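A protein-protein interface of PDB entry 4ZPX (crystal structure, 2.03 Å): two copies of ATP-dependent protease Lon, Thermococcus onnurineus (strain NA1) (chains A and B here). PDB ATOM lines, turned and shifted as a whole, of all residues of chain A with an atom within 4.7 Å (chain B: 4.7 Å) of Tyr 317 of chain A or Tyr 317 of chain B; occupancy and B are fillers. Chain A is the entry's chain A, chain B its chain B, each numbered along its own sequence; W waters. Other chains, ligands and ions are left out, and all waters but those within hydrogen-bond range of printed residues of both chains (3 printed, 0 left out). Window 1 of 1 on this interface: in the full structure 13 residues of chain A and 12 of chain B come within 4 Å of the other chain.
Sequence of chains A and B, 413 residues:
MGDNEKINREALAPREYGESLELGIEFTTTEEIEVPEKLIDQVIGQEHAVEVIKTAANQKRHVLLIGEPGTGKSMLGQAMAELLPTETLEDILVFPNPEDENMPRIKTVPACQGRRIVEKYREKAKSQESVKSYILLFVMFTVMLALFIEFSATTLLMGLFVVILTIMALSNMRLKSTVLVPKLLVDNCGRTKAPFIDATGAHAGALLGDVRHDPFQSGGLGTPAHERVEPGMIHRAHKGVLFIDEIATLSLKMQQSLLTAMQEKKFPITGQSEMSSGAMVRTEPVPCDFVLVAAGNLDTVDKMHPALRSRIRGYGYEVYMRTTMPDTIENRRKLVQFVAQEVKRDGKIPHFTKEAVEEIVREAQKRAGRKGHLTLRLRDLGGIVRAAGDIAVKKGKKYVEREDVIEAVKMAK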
ATOM      1  N   HIS A  48     -22.896  -0.844  33.159  1.00  0.00           N
ATOM      2  CA  HIS A  48     -23.784  -0.097  32.290  1.00  0.00           C
ATOM      3  C   HIS A  48     -22.931   0.730  31.310  1.00  0.00           C
ATOM      4  O   HIS A  48     -23.265   0.826  30.148  1.00  0.00           O
ATOM      5  CB  HIS A  48     -24.764   0.790  33.104  1.00  0.00           C
ATOM      6  CG  HIS A  48     -25.642   1.653  32.254  1.00  0.00           C
ATOM      7  ND1 HIS A  48     -26.578   1.131  31.383  1.00  0.00           N
ATOM      8  CD2 HIS A  48     -25.668   2.991  32.079  1.00  0.00           C
ATOM      9  CE1 HIS A  48     -27.169   2.117  30.733  1.00  0.00           C
ATOM     10  NE2 HIS A  48     -26.625   3.257  31.124  1.00  0.00           N
ATOM     11  N   GLU A  51     -21.812  -1.721  28.576  1.00  0.00           N
ATOM     12  CA  GLU A  51     -22.794  -2.121  27.554  1.00  0.00           C
ATOM     13  C   GLU A  51     -23.101  -0.873  26.620  1.00  0.00           C
ATOM     14  O   GLU A  51     -23.267  -1.040  25.393  1.00  0.00           O
ATOM     15  CB  GLU A  51     -24.045  -2.753  28.264  1.00  0.00           C
ATOM     16  CG  GLU A  51     -24.755  -1.726  29.106  1.00  0.00           C
ATOM     17  CD  GLU A  51     -25.946  -2.228  29.951  1.00  0.00           C
ATOM     18  OE1 GLU A  51     -26.243  -3.452  29.965  1.00  0.00           O
ATOM     19  OE2 GLU A  51     -26.572  -1.317  30.607  1.00  0.00           O
ATOM     20  N   VAL A  52     -23.117   0.349  27.173  1.00  0.00           N
ATOM     21  CA  VAL A  52     -23.282   1.596  26.382  1.00  0.00           C
ATOM     22  C   VAL A  52     -22.118   1.800  25.372  1.00  0.00           C
ATOM     23  O   VAL A  52     -22.331   2.058  24.167  1.00  0.00           O
ATOM     24  CB  VAL A  52     -23.433   2.877  27.300  1.00  0.00           C
ATOM     25  CG1 VAL A  52     -23.393   4.185  26.484  1.00  0.00           C
ATOM     26  CG2 VAL A  52     -24.708   2.819  28.127  1.00  0.00           C
ATOM     27  N   THR A  55     -22.587  -0.651  22.520  1.00  0.00           N
ATOM     28  CA  THR A  55     -23.681  -0.187  21.688  1.00  0.00           C
ATOM     29  C   THR A  55     -23.286   0.999  20.810  1.00  0.00           C
ATOM     30  O   THR A  55     -23.512   1.008  19.611  1.00  0.00           O
ATOM     31  CB  THR A  55     -24.845   0.231  22.562  1.00  0.00           C
ATOM     32  OG1 THR A  55     -25.165  -0.858  23.431  1.00  0.00           O
ATOM     33  CG2 THR A  55     -26.000   0.596  21.718  1.00  0.00           C
ATOM     34  N   ALA A  56     -22.605   1.942  21.409  1.00  0.00           N
ATOM     35  CA  ALA A  56     -22.205   3.131  20.731  1.00  0.00           C
ATOM     36  C   ALA A  56     -21.199   2.858  19.672  1.00  0.00           C
ATOM     37  O   ALA A  56     -21.230   3.501  18.632  1.00  0.00           O
ATOM     38  CB  ALA A  56     -21.666   4.173  21.698  1.00  0.00           C
ATOM     39  N   GLN A  59     -23.224   1.253  16.707  1.00  0.00           N
ATOM     40  CA  GLN A  59     -24.049   2.192  15.962  1.00  0.00           C
ATOM     41  C   GLN A  59     -23.249   3.438  15.510  1.00  0.00           C
ATOM     42  O   GLN A  59     -23.786   4.279  14.870  1.00  0.00           O
ATOM     43  CB  GLN A  59     -25.228   2.671  16.853  1.00  0.00           C
ATOM     44  CG  GLN A  59     -26.189   1.583  17.439  1.00  0.00           C
ATOM     45  CD  GLN A  59     -27.104   2.086  18.592  1.00  0.00           C
ATOM     46  OE1 GLN A  59     -28.083   1.415  18.963  1.00  0.00           O
ATOM     47  NE2 GLN A  59     -26.806   3.268  19.151  1.00  0.00           N
ATOM     48  N   ARG A  61     -21.993   6.108  17.701  1.00  0.00           N
ATOM     49  CA  ARG A  61     -22.613   7.235  18.348  1.00  0.00           C
ATOM     50  C   ARG A  61     -21.677   7.848  19.388  1.00  0.00           C
ATOM     51  O   ARG A  61     -20.947   7.138  20.054  1.00  0.00           O
ATOM     52  CB  ARG A  61     -23.936   6.798  19.006  1.00  0.00           C
ATOM     53  CG  ARG A  61     -24.948   6.113  18.076  1.00  0.00           C
ATOM     54  CD  ARG A  61     -25.646   7.100  17.173  1.00  0.00           C
ATOM     55  NE  ARG A  61     -26.484   6.445  16.157  1.00  0.00           N
ATOM     56  CZ  ARG A  61     -26.381   6.615  14.835  1.00  0.00           C
ATOM     57  NH1 ARG A  61     -25.471   7.408  14.268  1.00  0.00           N
ATOM     58  NH2 ARG A  61     -27.209   5.961  14.058  1.00  0.00           N
ATOM     59  N   HIS A  62     -21.807   9.149  19.595  1.00  0.00           N
ATOM     60  CA  HIS A  62     -20.967   9.877  20.485  1.00  0.00           C
ATOM     61  C   HIS A  62     -21.406   9.573  21.878  1.00  0.00           C
ATOM     62  O   HIS A  62     -22.560   9.197  22.108  1.00  0.00           O
ATOM     63  CB  HIS A  62     -21.110  11.369  20.226  1.00  0.00           C
ATOM     64  CG  HIS A  62     -20.874  11.739  18.821  1.00  0.00           C
ATOM     65  ND1 HIS A  62     -19.671  11.512  18.209  1.00  0.00           N
ATOM     66  CD2 HIS A  62     -21.693  12.243  17.874  1.00  0.00           C
ATOM     67  CE1 HIS A  62     -19.744  11.879  16.951  1.00  0.00           C
ATOM     68  NE2 HIS A  62     -20.970  12.315  16.719  1.00  0.00           N
ATOM     69  N   VAL A  63     -20.514   9.802  22.823  1.00  0.00           N
ATOM     70  CA  VAL A  63     -20.760   9.416  24.191  1.00  0.00           C
ATOM     71  C   VAL A  63     -20.165  10.456  25.083  1.00  0.00           C
ATOM     72  O   VAL A  63     -19.029  10.954  24.874  1.00  0.00           O
ATOM     73  CB  VAL A  63     -20.113   8.059  24.469  1.00  0.00           C
ATOM     74  CG1 VAL A  63     -20.165   7.665  25.964  1.00  0.00           C
ATOM     75  CG2 VAL A  63     -20.705   6.986  23.616  1.00  0.00           C
ATOM     76  N   LEU A  64     -20.957  10.878  26.049  1.00  0.00           N
ATOM     77  CA  LEU A  64     -20.447  11.669  27.130  1.00  0.00           C
ATOM     78  C   LEU A  64     -20.362  10.845  28.439  1.00  0.00           C
ATOM     79  O   LEU A  64     -21.364  10.381  28.985  1.00  0.00           O
ATOM     80  CB  LEU A  64     -21.290  12.940  27.288  1.00  0.00           C
ATOM     81  CG  LEU A  64     -21.036  13.749  28.535  1.00  0.00           C
ATOM     82  CD1 LEU A  64     -19.643  14.390  28.634  1.00  0.00           C
ATOM     83  CD2 LEU A  64     -22.040  14.868  28.510  1.00  0.00           C
ATOM     84  N   ILE A 312     -25.244  15.524  21.905  1.00  0.00           N
ATOM     85  CA  ILE A 312     -24.975  14.211  22.557  1.00  0.00           C
ATOM     86  C   ILE A 312     -26.285  13.577  23.064  1.00  0.00           C
ATOM     87  O   ILE A 312     -26.571  12.423  22.732  1.00  0.00           O
ATOM     88  CB  ILE A 312     -23.856  14.327  23.615  1.00  0.00           C
ATOM     89  CG1 ILE A 312     -22.575  14.732  22.845  1.00  0.00           C
ATOM     90  CG2 ILE A 312     -23.620  12.925  24.238  1.00  0.00           C
ATOM     91  CD1 ILE A 312     -21.477  15.326  23.673  1.00  0.00           C
ATOM     92  N   GLY A 316     -26.752  10.698  20.786  1.00  0.00           N
ATOM     93  CA  GLY A 316     -25.763   9.796  21.371  1.00  0.00           C
ATOM     94  C   GLY A 316     -26.115   9.348  22.769  1.00  0.00           C
ATOM     95  O   GLY A 316     -27.296   9.314  23.144  1.00  0.00           O
ATOM     96  N   TYR A 317     -25.097   9.100  23.600  1.00  0.00           N
ATOM     97  CA  TYR A 317     -25.319   8.510  24.938  1.00  0.00           C
ATOM     98  C   TYR A 317     -24.600   9.242  25.996  1.00  0.00           C
ATOM     99  O   TYR A 317     -23.383   9.528  25.871  1.00  0.00           O
ATOM    100  CB  TYR A 317     -24.858   7.059  24.943  1.00  0.00           C
ATOM    101  CG  TYR A 317     -25.664   6.196  24.039  1.00  0.00           C
ATOM    102  CD1 TYR A 317     -26.853   5.600  24.491  1.00  0.00           C
ATOM    103  CD2 TYR A 317     -25.294   5.974  22.728  1.00  0.00           C
ATOM    104  CE1 TYR A 317     -27.583   4.779  23.669  1.00  0.00           C
ATOM    105  CE2 TYR A 317     -26.060   5.183  21.920  1.00  0.00           C
ATOM    106  CZ  TYR A 317     -27.244   4.621  22.415  1.00  0.00           C
ATOM    107  OH  TYR A 317     -28.042   3.791  21.637  1.00  0.00           O
ATOM    108  N   GLU A 318     -25.323   9.531  27.068  1.00  0.00           N
ATOM    109  CA  GLU A 318     -24.792  10.043  28.301  1.00  0.00           C
ATOM    110  C   GLU A 318     -24.643   8.873  29.239  1.00  0.00           C
ATOM    111  O   GLU A 318     -25.606   8.144  29.397  1.00  0.00           O
ATOM    112  CB  GLU A 318     -25.787  11.006  28.905  1.00  0.00           C
ATOM    113  CG  GLU A 318     -25.194  12.319  29.232  1.00  0.00           C
ATOM    114  CD  GLU A 318     -26.169  13.491  29.408  1.00  0.00           C
ATOM    115  OE1 GLU A 318     -27.370  13.348  29.128  1.00  0.00           O
ATOM    116  OE2 GLU A 318     -25.718  14.567  29.852  1.00  0.00           O
ATOM    117  N   VAL A 319     -23.465   8.702  29.870  1.00  0.00           N
ATOM    118  CA  VAL A 319     -23.276   7.683  30.917  1.00  0.00           C
ATOM    119  C   VAL A 319     -22.857   8.280  32.239  1.00  0.00           C
ATOM    120  O   VAL A 319     -21.885   9.054  32.313  1.00  0.00           O
ATOM    121  CB  VAL A 319     -22.187   6.736  30.502  1.00  0.00           C
ATOM    122  CG1 VAL A 319     -22.054   5.647  31.520  1.00  0.00           C
ATOM    123  CG2 VAL A 319     -22.494   6.184  29.124  1.00  0.00           C
ATOM    124  N   HIS B  48     -33.118   8.081  16.987  1.00  0.00           N
ATOM    125  CA  HIS B  48     -32.254   7.777  18.111  1.00  0.00           C
ATOM    126  C   HIS B  48     -33.049   7.076  19.203  1.00  0.00           C
ATOM    127  O   HIS B  48     -32.617   6.067  19.711  1.00  0.00           O
ATOM    128  CB  HIS B  48     -31.597   9.043  18.664  1.00  0.00           C
ATOM    129  CG  HIS B  48     -30.622   8.755  19.768  1.00  0.00           C
ATOM    130  ND1 HIS B  48     -29.627   7.799  19.644  1.00  0.00           N
ATOM    131  CD2 HIS B  48     -30.504   9.268  21.010  1.00  0.00           C
ATOM    132  CE1 HIS B  48     -28.942   7.739  20.773  1.00  0.00           C
ATOM    133  NE2 HIS B  48     -29.464   8.607  21.622  1.00  0.00           N
ATOM    134  N   GLU B  51     -33.462   3.546  18.207  1.00  0.00           N
ATOM    135  CA  GLU B  51     -32.311   2.654  18.368  1.00  0.00           C
ATOM    136  C   GLU B  51     -31.960   2.424  19.886  1.00  0.00           C
ATOM    137  O   GLU B  51     -31.447   1.365  20.242  1.00  0.00           O
ATOM    138  CB  GLU B  51     -31.146   3.147  17.515  1.00  0.00           C
ATOM    139  CG  GLU B  51     -30.327   4.245  18.110  1.00  0.00           C
ATOM    140  CD  GLU B  51     -29.288   4.764  17.110  1.00  0.00           C
ATOM    141  OE1 GLU B  51     -28.877   4.008  16.176  1.00  0.00           O
ATOM    142  OE2 GLU B  51     -28.896   5.932  17.280  1.00  0.00           O
ATOM    143  N   VAL B  52     -32.349   3.339  20.759  1.00  0.00           N
ATOM    144  CA  VAL B  52     -32.240   3.135  22.230  1.00  0.00           C
ATOM    145  C   VAL B  52     -33.249   2.142  22.769  1.00  0.00           C
ATOM    146  O   VAL B  52     -32.918   1.306  23.639  1.00  0.00           O
ATOM    147  CB  VAL B  52     -32.363   4.464  22.993  1.00  0.00           C
ATOM    148  CG1 VAL B  52     -32.253   4.269  24.499  1.00  0.00           C
ATOM    149  CG2 VAL B  52     -31.307   5.426  22.530  1.00  0.00           C
ATOM    150  N   THR B  55     -32.066  -1.353  21.903  1.00  0.00           N
ATOM    151  CA  THR B  55     -30.954  -1.693  22.786  1.00  0.00           C
ATOM    152  C   THR B  55     -31.487  -2.064  24.150  1.00  0.00           C
ATOM    153  O   THR B  55     -31.178  -3.106  24.692  1.00  0.00           O
ATOM    154  CB  THR B  55     -29.981  -0.499  22.932  1.00  0.00           C
ATOM    155  OG1 THR B  55     -29.504  -0.137  21.646  1.00  0.00           O
ATOM    156  CG2 THR B  55     -28.770  -0.839  23.750  1.00  0.00           C
ATOM    157  N   ALA B  56     -32.319  -1.187  24.687  1.00  0.00           N
ATOM    158  CA  ALA B  56     -32.904  -1.388  25.971  1.00  0.00           C
ATOM    159  C   ALA B  56     -33.783  -2.643  26.062  1.00  0.00           C
ATOM    160  O   ALA B  56     -33.775  -3.331  27.095  1.00  0.00           O
ATOM    161  CB  ALA B  56     -33.662  -0.122  26.398  1.00  0.00           C
ATOM    162  N   GLN B  59     -31.277  -5.489  26.147  1.00  0.00           N
ATOM    163  CA  GLN B  59     -30.531  -5.634  27.384  1.00  0.00           C
ATOM    164  C   GLN B  59     -31.459  -5.755  28.616  1.00  0.00           C
ATOM    165  O   GLN B  59     -30.991  -5.984  29.716  1.00  0.00           O
ATOM    166  CB  GLN B  59     -29.600  -4.412  27.551  1.00  0.00           C
ATOM    167  CG  GLN B  59     -28.518  -4.185  26.454  1.00  0.00           C
ATOM    168  CD  GLN B  59     -27.787  -2.832  26.548  1.00  0.00           C
ATOM    169  OE1 GLN B  59     -26.733  -2.644  25.924  1.00  0.00           O
ATOM    170  NE2 GLN B  59     -28.309  -1.902  27.342  1.00  0.00           N
ATOM    171  N   ARG B  61     -33.403  -2.989  29.987  1.00  0.00           N
ATOM    172  CA  ARG B  61     -33.036  -1.880  30.810  1.00  0.00           C
ATOM    173  C   ARG B  61     -34.164  -0.907  30.842  1.00  0.00           C
ATOM    174  O   ARG B  61     -34.848  -0.682  29.844  1.00  0.00           O
ATOM    175  CB  ARG B  61     -31.802  -1.117  30.275  1.00  0.00           C
ATOM    176  CG  ARG B  61     -30.520  -1.918  30.194  1.00  0.00           C
ATOM    177  CD  ARG B  61     -30.216  -2.529  31.535  1.00  0.00           C
ATOM    178  NE  ARG B  61     -28.931  -3.230  31.559  1.00  0.00           N
ATOM    179  CZ  ARG B  61     -28.773  -4.459  32.017  1.00  0.00           C
ATOM    180  NH1 ARG B  61     -29.812  -5.200  32.386  1.00  0.00           N
ATOM    181  NH2 ARG B  61     -27.566  -4.973  32.050  1.00  0.00           N
ATOM    182  N   HIS B  62     -34.265  -0.217  31.948  1.00  0.00           N
ATOM    183  CA  HIS B  62     -35.287   0.816  32.086  1.00  0.00           C
ATOM    184  C   HIS B  62     -35.037   2.064  31.225  1.00  0.00           C
ATOM    185  O   HIS B  62     -33.868   2.356  30.888  1.00  0.00           O
ATOM    186  CB  HIS B  62     -35.377   1.216  33.540  1.00  0.00           C
ATOM    187  CG  HIS B  62     -35.507   0.070  34.466  1.00  0.00           C
ATOM    188  ND1 HIS B  62     -36.537  -0.833  34.373  1.00  0.00           N
ATOM    189  CD2 HIS B  62     -34.744  -0.329  35.510  1.00  0.00           C
ATOM    190  CE1 HIS B  62     -36.414  -1.741  35.326  1.00  0.00           C
ATOM    191  NE2 HIS B  62     -35.329  -1.466  36.023  1.00  0.00           N
ATOM    192  N   VAL B  63     -36.091   2.855  30.941  1.00  0.00           N
ATOM    193  CA  VAL B  63     -35.962   4.020  30.092  1.00  0.00           C
ATOM    194  C   VAL B  63     -36.833   5.144  30.594  1.00  0.00           C
ATOM    195  O   VAL B  63     -37.992   4.908  31.070  1.00  0.00           O
ATOM    196  CB  VAL B  63     -36.463   3.700  28.692  1.00  0.00           C
ATOM    197  CG1 VAL B  63     -36.465   5.003  27.851  1.00  0.00           C
ATOM    198  CG2 VAL B  63     -35.602   2.632  28.032  1.00  0.00           C
ATOM    199  N   LEU B  64     -36.286   6.343  30.575  1.00  0.00           N
ATOM    200  CA  LEU B  64     -37.028   7.574  30.790  1.00  0.00           C
ATOM    201  C   LEU B  64     -37.135   8.300  29.468  1.00  0.00           C
ATOM    202  O   LEU B  64     -36.121   8.697  28.869  1.00  0.00           O
ATOM    203  CB  LEU B  64     -36.359   8.454  31.803  1.00  0.00           C
ATOM    204  CG  LEU B  64     -37.003   9.796  32.107  1.00  0.00           C
ATOM    205  CD1 LEU B  64     -38.394   9.616  32.642  1.00  0.00           C
ATOM    206  CD2 LEU B  64     -36.162  10.500  33.154  1.00  0.00           C
ATOM    207  N   ILE B 312     -32.338   5.385  36.907  1.00  0.00           N
ATOM    208  CA  ILE B 312     -32.440   5.303  35.453  1.00  0.00           C
ATOM    209  C   ILE B 312     -31.102   5.749  34.795  1.00  0.00           C
ATOM    210  O   ILE B 312     -30.563   5.039  33.956  1.00  0.00           O
ATOM    211  CB  ILE B 312     -33.678   6.051  34.937  1.00  0.00           C
ATOM    212  CG1 ILE B 312     -34.957   5.334  35.453  1.00  0.00           C
ATOM    213  CG2 ILE B 312     -33.746   6.004  33.408  1.00  0.00           C
ATOM    214  CD1 ILE B 312     -36.190   6.172  35.330  1.00  0.00           C
ATOM    215  N   GLY B 316     -29.954   2.665  33.272  1.00  0.00           N
ATOM    216  CA  GLY B 316     -30.937   2.627  32.157  1.00  0.00           C
ATOM    217  C   GLY B 316     -30.621   3.677  31.102  1.00  0.00           C
ATOM    218  O   GLY B 316     -29.451   4.018  30.895  1.00  0.00           O
ATOM    219  N   TYR B 317     -31.620   4.165  30.377  1.00  0.00           N
ATOM    220  CA  TYR B 317     -31.403   5.178  29.330  1.00  0.00           C
ATOM    221  C   TYR B 317     -32.360   6.307  29.498  1.00  0.00           C
ATOM    222  O   TYR B 317     -33.575   6.066  29.627  1.00  0.00           O
ATOM    223  CB  TYR B 317     -31.582   4.546  27.979  1.00  0.00           C
ATOM    224  CG  TYR B 317     -30.566   3.501  27.674  1.00  0.00           C
ATOM    225  CD1 TYR B 317     -29.303   3.849  27.149  1.00  0.00           C
ATOM    226  CD2 TYR B 317     -30.805   2.195  27.898  1.00  0.00           C
ATOM    227  CE1 TYR B 317     -28.367   2.884  26.883  1.00  0.00           C
ATOM    228  CE2 TYR B 317     -29.864   1.228  27.626  1.00  0.00           C
ATOM    229  CZ  TYR B 317     -28.630   1.593  27.156  1.00  0.00           C
ATOM    230  OH  TYR B 317     -27.697   0.626  26.794  1.00  0.00           O
ATOM    231  N   GLU B 318     -31.863   7.532  29.561  1.00  0.00           N
ATOM    232  CA  GLU B 318     -32.688   8.732  29.480  1.00  0.00           C
ATOM    233  C   GLU B 318     -32.781   8.917  27.963  1.00  0.00           C
ATOM    234  O   GLU B 318     -31.754   8.748  27.289  1.00  0.00           O
ATOM    235  CB  GLU B 318     -32.033   9.971  30.084  1.00  0.00           C
ATOM    236  CG  GLU B 318     -32.009  10.110  31.599  1.00  0.00           C
ATOM    237  CD  GLU B 318     -31.882  11.577  32.108  1.00  0.00           C
ATOM    238  OE1 GLU B 318     -31.442  12.471  31.365  1.00  0.00           O
ATOM    239  OE2 GLU B 318     -32.218  11.883  33.281  1.00  0.00           O
ATOM    240  N   VAL B 319     -33.971   9.189  27.416  1.00  0.00           N
ATOM    241  CA  VAL B 319     -34.127   9.481  25.999  1.00  0.00           C
ATOM    242  C   VAL B 319     -34.790  10.857  25.814  1.00  0.00           C
ATOM    243  O   VAL B 319     -35.953  11.058  26.183  1.00  0.00           O
ATOM    244  CB  VAL B 319     -34.948   8.438  25.263  1.00  0.00           C
ATOM    245  CG1 VAL B 319     -35.067   8.827  23.803  1.00  0.00           C
ATOM    246  CG2 VAL B 319     -34.284   7.071  25.327  1.00  0.00           C
HETATM  247  O   HOH W   1     -28.497   8.810  16.807  1.00  0.00           O
HETATM  248  O   HOH W   2     -24.044  -3.689  24.518  1.00  0.00           O
HETATM  249  O   HOH W   3     -30.016  -0.937  18.482  1.00  0.00           O
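Water W2 lies within hydrogen-bond range of O of Glu 51 of chain A (2.9 Å), OE1 of Gln 59 of chain B (3.2 Å) and OG1 of Thr 55 of chain A (3.2 Å).
Water W1 lies within hydrogen-bond range of OE2 of Glu 51 of chain B, NE of Arg 61 of chain A and ND1 of His 48 of chain B.
Water W3 lies within hydrogen-bond range of the side-chain amide oxygen of Gln 59 of chain A (3.1 Å), the backbone carbonyl oxygen of Glu 51 of chain B (3.2 Å) and the side-chain hydroxyl of Thr 55 of chain B (3.3 Å).
NE2 of Gln 59 of chain A is in hydrogen-bond range of OH of Tyr 317 of chain A (2.8 Å).
The backbone NH of Tyr 317 of chain A sits at hydrogen-bond distance from the backbone carbonyl oxygen of His 62 of chain A, at 2.9 Å.
A ring nitrogen (ND1) of His 48 of chain B lies within hydrogen-bond range of the side-chain carboxylate (OE2) of Glu 51 of chain B (3.1 Å).
O of Ala 56 of chain B sits at hydrogen-bond distance from N of Arg 61 of chain B.
NE2 of Gln 59 of chain B is in hydrogen-bond range of OH of Tyr 317 of chain B (2.7 Å).
O of His 62 of chain B sits at hydrogen-bond distance from N of Tyr 317 of chain B (2.9 Å).
NE2 of His 48 of chain A is in hydrogen-bond range of O of Gly 316 of chain B (2.9 Å).
The side-chain carboxylate of Glu 51 of chain A lies within salt-bridge range of the guanidinium group of Arg 61 of chain B (2.9 Å).
The side-chain amide oxygen (OE1) of Gln 59 of chain B is in hydrogen-bond range of the side-chain hydroxyl (OG1) of Thr 55 of chain A.
The side-chain amide oxygen of Gln 59 of chain A sits at hydrogen-bond distance from the side-chain hydroxyl of Thr 55 of chain B (3.4 Å).
The guanidinium group of Arg 61 of chain A is in salt-bridge range of the side-chain carboxylate of Glu 51 of chain B (2.7 Å).
The backbone carbonyl oxygen of Gly 316 of chain A is in hydrogen-bond range of a ring nitrogen (NE2) of His 48 of chain B (2.7 Å).
Tyr 317 of chain A touches just these residues of chain B: His 48 (3.9 Å), Val 52 (3.8 Å) and Tyr 317 (3.8 Å).
Tyr 317 of chain B touches three residues of chain A.
Printed residues of chain A within 4 Å of Gln 59 of chain B: Glu 51 and Thr 55.
Printed residues of chain B within 4 Å of Glu 51 of chain A: Gln 59 (3.5 Å) and Arg 61 (2.9 Å).
Leu 64 of chain B touches none of the printed residues of chain A.
Glu 318 of chain B touches none of the printed residues of chain A.
The nearest residue of chain B that does not touch Tyr 317 of chain A is Thr 55 of chain B (4.2 Å).
The nearest residue of chain A that does not touch Tyr 317 of chain B is Glu 51 of chain A (4.4 Å).
Hydrophobic or aromatic side chains of chain A that line the printed part of chain B: His 48, Val 52 and Tyr 317.
Printed residues of chain B that touch a printed residue of chain A: His 48, Glu 51, Val 52, Thr 55, Gln 59, Arg 61, Gly 316 and Tyr 317.
Among the printed residues, 14 pairs touch across the chains.
Among the printed residues, Asp or Glu carboxylates within 4 Å of a Lys or Arg side-chain nitrogen of the other chain: Glu 51 of chain A with Arg 61 of chain B (2.9 Å) and Arg 61 of chain A with Glu 51 of chain B (2.7 Å).
His 48 of chain A touches Gly 316 of chain B, and with the chains exchanged Gly 316 of chain A touches His 48 of chain B.
Glu 51 of chain A touches Gln 59 of chain B, and with the chains exchanged Gln 59 of chain A touches Glu 51 of chain B.
Val 52 of chain A touches Tyr 317 of chain B, and with the chains exchanged Tyr 317 of chain A touches Val 52 of chain B.
Tyr 317 of chain A touches its own counterpart, Tyr 317 of chain B.
Positions printed for both chains: 48, 51, 52, 55, 56, 59, 61, 62, 63, 64, 312, 316, 317, 318 and 319.
Among the printed residues, merely in contact across the chains: His 48 of chain A with Tyr 317 of chain B (3.9 Å), Glu 51 of chain A with Gln 59 of chain B (3.5 Å), Val 52 of chain A with Tyr 317 of chain B (3.9 Å), Thr 55 of chain A with Thr 55 of chain B (3.6 Å), Gln 59 of chain A with Glu 51 of chain B (3.5 Å), Tyr 317 of chain A with His 48 of chain B (3.9 Å), Tyr 317 of chain A with Val 52 of chain B (3.8 Å) and Tyr 317 of chain A with Tyr 317 of chain B (3.8 Å).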
